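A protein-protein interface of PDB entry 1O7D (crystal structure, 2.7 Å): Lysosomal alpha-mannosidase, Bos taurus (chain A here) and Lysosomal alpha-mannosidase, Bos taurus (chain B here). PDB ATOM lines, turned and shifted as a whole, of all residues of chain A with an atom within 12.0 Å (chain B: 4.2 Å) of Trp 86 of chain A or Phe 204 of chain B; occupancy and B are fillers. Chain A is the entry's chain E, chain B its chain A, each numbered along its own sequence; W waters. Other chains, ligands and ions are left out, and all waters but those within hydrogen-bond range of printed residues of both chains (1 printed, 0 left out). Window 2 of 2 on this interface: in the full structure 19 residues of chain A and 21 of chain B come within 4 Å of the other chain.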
ATOM      1  N   SER A  82       9.317 -35.343  14.237  1.00  0.00           N
ATOM      2  CA  SER A  82      10.224 -34.249  14.544  1.00  0.00           C
ATOM      3  C   SER A  82      10.344 -33.331  13.337  1.00  0.00           C
ATOM      4  O   SER A  82      10.133 -33.751  12.201  1.00  0.00           O
ATOM      5  CB  SER A  82      11.615 -34.789  14.926  1.00  0.00           C
ATOM      6  OG  SER A  82      12.184 -35.581  13.889  1.00  0.00           O
ATOM      7  N   ARG A  83      10.689 -32.079  13.592  1.00  0.00           N
ATOM      8  CA  ARG A  83      10.849 -31.084  12.541  1.00  0.00           C
ATOM      9  C   ARG A  83      12.229 -30.442  12.633  1.00  0.00           C
ATOM     10  O   ARG A  83      12.820 -30.423  13.702  1.00  0.00           O
ATOM     11  CB  ARG A  83       9.778 -30.012  12.704  1.00  0.00           C
ATOM     12  CG  ARG A  83       8.409 -30.413  12.184  1.00  0.00           C
ATOM     13  CD  ARG A  83       7.306 -29.858  13.083  1.00  0.00           C
ATOM     14  NE  ARG A  83       7.559 -28.487  13.532  1.00  0.00           N
ATOM     15  CZ  ARG A  83       7.418 -27.401  12.777  1.00  0.00           C
ATOM     16  NH1 ARG A  83       7.021 -27.492  11.517  1.00  0.00           N
ATOM     17  NH2 ARG A  83       7.677 -26.209  13.285  1.00  0.00           N
ATOM     18  N   LEU A  84      12.741 -29.915  11.527  1.00  0.00           N
ATOM     19  CA  LEU A  84      14.053 -29.277  11.536  1.00  0.00           C
ATOM     20  C   LEU A  84      13.991 -28.049  12.442  1.00  0.00           C
ATOM     21  O   LEU A  84      12.940 -27.419  12.559  1.00  0.00           O
ATOM     22  CB  LEU A  84      14.428 -28.832  10.126  1.00  0.00           C
ATOM     23  CG  LEU A  84      14.239 -29.804   8.963  1.00  0.00           C
ATOM     24  CD1 LEU A  84      14.707 -29.128   7.672  1.00  0.00           C
ATOM     25  CD2 LEU A  84      15.020 -31.072   9.207  1.00  0.00           C
ATOM     26  N   GLN A  85      15.095 -27.697  13.089  1.00  0.00           N
ATOM     27  CA  GLN A  85      15.075 -26.514  13.948  1.00  0.00           C
ATOM     28  C   GLN A  85      15.551 -25.271  13.195  1.00  0.00           C
ATOM     29  O   GLN A  85      16.219 -25.391  12.172  1.00  0.00           O
ATOM     30  CB  GLN A  85      15.917 -26.765  15.193  1.00  0.00           C
ATOM     31  CG  GLN A  85      15.387 -27.905  16.041  1.00  0.00           C
ATOM     32  CD  GLN A  85      14.091 -27.573  16.709  1.00  0.00           C
ATOM     33  OE1 GLN A  85      14.042 -26.862  17.799  1.00  0.00           O
ATOM     34  NE2 GLN A  85      12.978 -28.061  16.115  1.00  0.00           N
ATOM     35  N   TRP A  86      15.187 -24.089  13.685  1.00  0.00           N
ATOM     36  CA  TRP A  86      15.569 -22.841  13.027  1.00  0.00           C
ATOM     37  C   TRP A  86      15.916 -21.715  14.003  1.00  0.00           C
ATOM     38  O   TRP A  86      15.116 -21.352  14.874  1.00  0.00           O
ATOM     39  CB  TRP A  86      14.444 -22.369  12.097  1.00  0.00           C
ATOM     40  CG  TRP A  86      14.150 -23.318  11.007  1.00  0.00           C
ATOM     41  CD1 TRP A  86      13.197 -24.280  11.005  1.00  0.00           C
ATOM     42  CD2 TRP A  86      14.869 -23.458   9.784  1.00  0.00           C
ATOM     43  NE1 TRP A  86      13.275 -25.021   9.855  1.00  0.00           N
ATOM     44  CE2 TRP A  86      14.298 -24.536   9.088  1.00  0.00           C
ATOM     45  CE3 TRP A  86      15.945 -22.775   9.210  1.00  0.00           C
ATOM     46  CZ2 TRP A  86      14.770 -24.955   7.843  1.00  0.00           C
ATOM     47  CZ3 TRP A  86      16.411 -23.188   7.979  1.00  0.00           C
ATOM     48  CH2 TRP A  86      15.826 -24.269   7.307  1.00  0.00           C
ATOM     49  N   THR A  87      17.102 -21.144  13.847  1.00  0.00           N
ATOM     50  CA  THR A  87      17.530 -20.063  14.731  1.00  0.00           C
ATOM     51  C   THR A  87      17.018 -18.725  14.249  1.00  0.00           C
ATOM     52  O   THR A  87      17.354 -18.296  13.148  1.00  0.00           O
ATOM     53  CB  THR A  87      19.071 -19.944  14.798  1.00  0.00           C
ATOM     54  OG1 THR A  87      19.631 -21.166  15.276  1.00  0.00           O
ATOM     55  CG2 THR A  87      19.482 -18.809  15.726  1.00  0.00           C
ATOM     56  N   THR A  88      16.221 -18.059  15.074  1.00  0.00           N
ATOM     57  CA  THR A  88      15.721 -16.742  14.715  1.00  0.00           C
ATOM     58  C   THR A  88      16.496 -15.729  15.549  1.00  0.00           C
ATOM     59  O   THR A  88      16.753 -15.980  16.723  1.00  0.00           O
ATOM     60  CB  THR A  88      14.224 -16.622  15.013  1.00  0.00           C
ATOM     61  OG1 THR A  88      13.996 -16.787  16.421  1.00  0.00           O
ATOM     62  CG2 THR A  88      13.448 -17.690  14.235  1.00  0.00           C
ATOM     63  N   ASP A  89      16.890 -14.608  14.944  1.00  0.00           N
ATOM     64  CA  ASP A  89      17.646 -13.565  15.649  1.00  0.00           C
ATOM     65  C   ASP A  89      16.763 -12.403  16.060  1.00  0.00           C
ATOM     66  O   ASP A  89      15.545 -12.498  15.976  1.00  0.00           O
ATOM     67  CB  ASP A  89      18.797 -13.040  14.782  1.00  0.00           C
ATOM     68  CG  ASP A  89      18.351 -12.651  13.378  1.00  0.00           C
ATOM     69  OD1 ASP A  89      17.470 -11.765  13.236  1.00  0.00           O
ATOM     70  OD2 ASP A  89      18.892 -13.237  12.409  1.00  0.00           O
ATOM     71  N   ASP B 165       8.384 -28.903   7.634  1.00  0.00           N
ATOM     72  CA  ASP B 165       9.591 -28.137   7.982  1.00  0.00           C
ATOM     73  C   ASP B 165       9.635 -26.790   7.293  1.00  0.00           C
ATOM     74  O   ASP B 165      10.015 -25.784   7.895  1.00  0.00           O
ATOM     75  CB  ASP B 165      10.854 -28.920   7.615  1.00  0.00           C
ATOM     76  CG  ASP B 165      10.870 -30.297   8.219  1.00  0.00           C
ATOM     77  OD1 ASP B 165      10.608 -30.388   9.435  1.00  0.00           O
ATOM     78  OD2 ASP B 165      11.138 -31.279   7.489  1.00  0.00           O
ATOM     79  N   GLY B 166       9.256 -26.786   6.022  1.00  0.00           N
ATOM     80  CA  GLY B 166       9.244 -25.557   5.257  1.00  0.00           C
ATOM     81  C   GLY B 166       7.976 -25.346   4.451  1.00  0.00           C
ATOM     82  O   GLY B 166       7.150 -26.265   4.284  1.00  0.00           O
ATOM     83  N   PHE B 167       7.851 -24.124   3.932  1.00  0.00           N
ATOM     84  CA  PHE B 167       6.708 -23.684   3.134  1.00  0.00           C
ATOM     85  C   PHE B 167       7.200 -22.630   2.118  1.00  0.00           C
ATOM     86  O   PHE B 167       7.786 -21.609   2.503  1.00  0.00           O
ATOM     87  CB  PHE B 167       5.677 -23.092   4.095  1.00  0.00           C
ATOM     88  CG  PHE B 167       4.531 -22.392   3.439  1.00  0.00           C
ATOM     89  CD1 PHE B 167       3.588 -23.095   2.700  1.00  0.00           C
ATOM     90  CD2 PHE B 167       4.333 -21.039   3.660  1.00  0.00           C
ATOM     91  CE1 PHE B 167       2.446 -22.456   2.202  1.00  0.00           C
ATOM     92  CE2 PHE B 167       3.204 -20.389   3.171  1.00  0.00           C
ATOM     93  CZ  PHE B 167       2.257 -21.095   2.443  1.00  0.00           C
ATOM     94  N   GLN B 188      12.761 -16.300   5.522  1.00  0.00           N
ATOM     95  CA  GLN B 188      12.745 -16.074   6.962  1.00  0.00           C
ATOM     96  C   GLN B 188      11.867 -17.083   7.689  1.00  0.00           C
ATOM     97  O   GLN B 188      11.387 -18.040   7.089  1.00  0.00           O
ATOM     98  CB  GLN B 188      12.276 -14.652   7.280  1.00  0.00           C
ATOM     99  CG  GLN B 188      10.825 -14.347   6.931  1.00  0.00           C
ATOM    100  CD  GLN B 188      10.428 -12.909   7.289  1.00  0.00           C
ATOM    101  OE1 GLN B 188      10.940 -11.954   6.723  1.00  0.00           O
ATOM    102  NE2 GLN B 188       9.528 -12.765   8.241  1.00  0.00           N
ATOM    103  N   VAL B 189      11.678 -16.876   8.988  1.00  0.00           N
ATOM    104  CA  VAL B 189      10.867 -17.772   9.800  1.00  0.00           C
ATOM    105  C   VAL B 189       9.568 -17.089  10.156  1.00  0.00           C
ATOM    106  O   VAL B 189       9.557 -15.971  10.676  1.00  0.00           O
ATOM    107  CB  VAL B 189      11.599 -18.180  11.082  1.00  0.00           C
ATOM    108  CG1 VAL B 189      10.619 -18.749  12.087  1.00  0.00           C
ATOM    109  CG2 VAL B 189      12.654 -19.213  10.747  1.00  0.00           C
ATOM    110  N   ASP B 202       6.155 -22.249  14.310  1.00  0.00           N
ATOM    111  CA  ASP B 202       7.221 -21.602  13.551  1.00  0.00           C
ATOM    112  C   ASP B 202       7.499 -22.373  12.281  1.00  0.00           C
ATOM    113  O   ASP B 202       8.123 -23.429  12.293  1.00  0.00           O
ATOM    114  CB  ASP B 202       8.487 -21.454  14.408  1.00  0.00           C
ATOM    115  CG  ASP B 202       8.351 -20.354  15.472  1.00  0.00           C
ATOM    116  OD1 ASP B 202       7.398 -19.550  15.381  1.00  0.00           O
ATOM    117  OD2 ASP B 202       9.197 -20.275  16.392  1.00  0.00           O
ATOM    118  N   LEU B 203       7.012 -21.828  11.178  1.00  0.00           N
ATOM    119  CA  LEU B 203       7.165 -22.443   9.875  1.00  0.00           C
ATOM    120  C   LEU B 203       8.173 -21.651   9.040  1.00  0.00           C
ATOM    121  O   LEU B 203       8.063 -20.432   8.909  1.00  0.00           O
ATOM    122  CB  LEU B 203       5.807 -22.466   9.177  1.00  0.00           C
ATOM    123  CG  LEU B 203       5.649 -23.341   7.940  1.00  0.00           C
ATOM    124  CD1 LEU B 203       5.930 -24.777   8.310  1.00  0.00           C
ATOM    125  CD2 LEU B 203       4.241 -23.228   7.384  1.00  0.00           C
ATOM    126  N   PHE B 204       9.165 -22.339   8.487  1.00  0.00           N
ATOM    127  CA  PHE B 204      10.159 -21.662   7.663  1.00  0.00           C
ATOM    128  C   PHE B 204       9.489 -21.254   6.346  1.00  0.00           C
ATOM    129  O   PHE B 204       8.697 -22.014   5.791  1.00  0.00           O
ATOM    130  CB  PHE B 204      11.353 -22.580   7.388  1.00  0.00           C
ATOM    131  CG  PHE B 204      12.543 -21.849   6.875  1.00  0.00           C
ATOM    132  CD1 PHE B 204      13.204 -20.931   7.683  1.00  0.00           C
ATOM    133  CD2 PHE B 204      12.946 -21.992   5.559  1.00  0.00           C
ATOM    134  CE1 PHE B 204      14.232 -20.162   7.182  1.00  0.00           C
ATOM    135  CE2 PHE B 204      13.980 -21.222   5.049  1.00  0.00           C
ATOM    136  CZ  PHE B 204      14.621 -20.305   5.864  1.00  0.00           C
ATOM    137  N   THR B 205       9.804 -20.070   5.835  1.00  0.00           N
ATOM    138  CA  THR B 205       9.157 -19.610   4.605  1.00  0.00           C
ATOM    139  C   THR B 205      10.105 -19.071   3.541  1.00  0.00           C
ATOM    140  O   THR B 205      11.008 -18.294   3.839  1.00  0.00           O
ATOM    141  CB  THR B 205       8.123 -18.506   4.914  1.00  0.00           C
ATOM    142  OG1 THR B 205       7.355 -18.880   6.061  1.00  0.00           O
ATOM    143  CG2 THR B 205       7.173 -18.325   3.745  1.00  0.00           C
HETATM  144  O   HOH W   1      11.144 -27.484  10.427  1.00  0.00           O
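N of Leu 84 of chain A sits at hydrogen-bond distance from OD1 of Asp 165 of chain B, 3.0 Å away. O of Asp 202 of chain B is in hydrogen-bond range of NH2 of Arg 83 of chain A (3.0 Å).
The backbone carbonyl oxygen of Arg 83 of chain A sits at hydrogen-bond distance from the side-chain amide nitrogen of Gln 85 of chain A (3.4 Å). O of Phe 204 of chain B sits at hydrogen-bond distance from N of Phe 167 of chain B (2.9 Å).
Asp 165 of chain B touches Arg 83 of chain A. Trp 86 of chain A touches Asp 165 of chain B. CB of Trp 86 of chain A touches CG2 of Val 189 of chain B, 3.9 Å away. CE3 of Trp 86 of chain A touches CD1 of Phe 204 of chain B, at 3.6 Å. Val 189 of chain B touches Thr 88 of chain A.
Of the printed residues of chain B, Arg 83 of chain A touches Asp 165 and Asp 202. Printed residues of chain B within 4 Å of Leu 84 of chain A: Asp 165 (3.0 Å). Gln 85 of chain A touches none of the printed residues of chain B. Trp 86 of chain A touches three residues of chain B. Asp 89 of chain A touches none of the printed residues of chain B. Asp 165 of chain B touches just these residues of chain A: Arg 83, Leu 84 and Trp 86. No residue of chain A comes within 4 Å of Phe 167 of chain B. Val 189 of chain B touches two residues of chain A. No residue of chain A comes within 4 Å of Leu 203 of chain B. Phe 204 of chain B touches just one residue of chain A: Trp 86. No residue of chain A comes within 4 Å of Thr 205 of chain B. The nearest residue of chain A that does not touch Phe 204 of chain B is Arg 83 of chain A (6.3 Å).
Printed residues of chain B that touch a printed residue of chain A: Asp 165, Val 189, Asp 202 and Phe 204. Hydrophobic or aromatic side chains of chain B that line the printed part of chain A: Val 189 and Phe 204. Hydrophobic or aromatic side chains of chain A within 4 Å of the printed part of chain B: Leu 84 and Trp 86.
Water W1 lies within hydrogen-bond range of the backbone carbonyl oxygen of Leu 84 of chain A (2.8 Å), the side-chain carboxylate of Asp 165 of chain B (3.1 Å) and the indole nitrogen of Trp 86 of chain A (3.3 Å).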
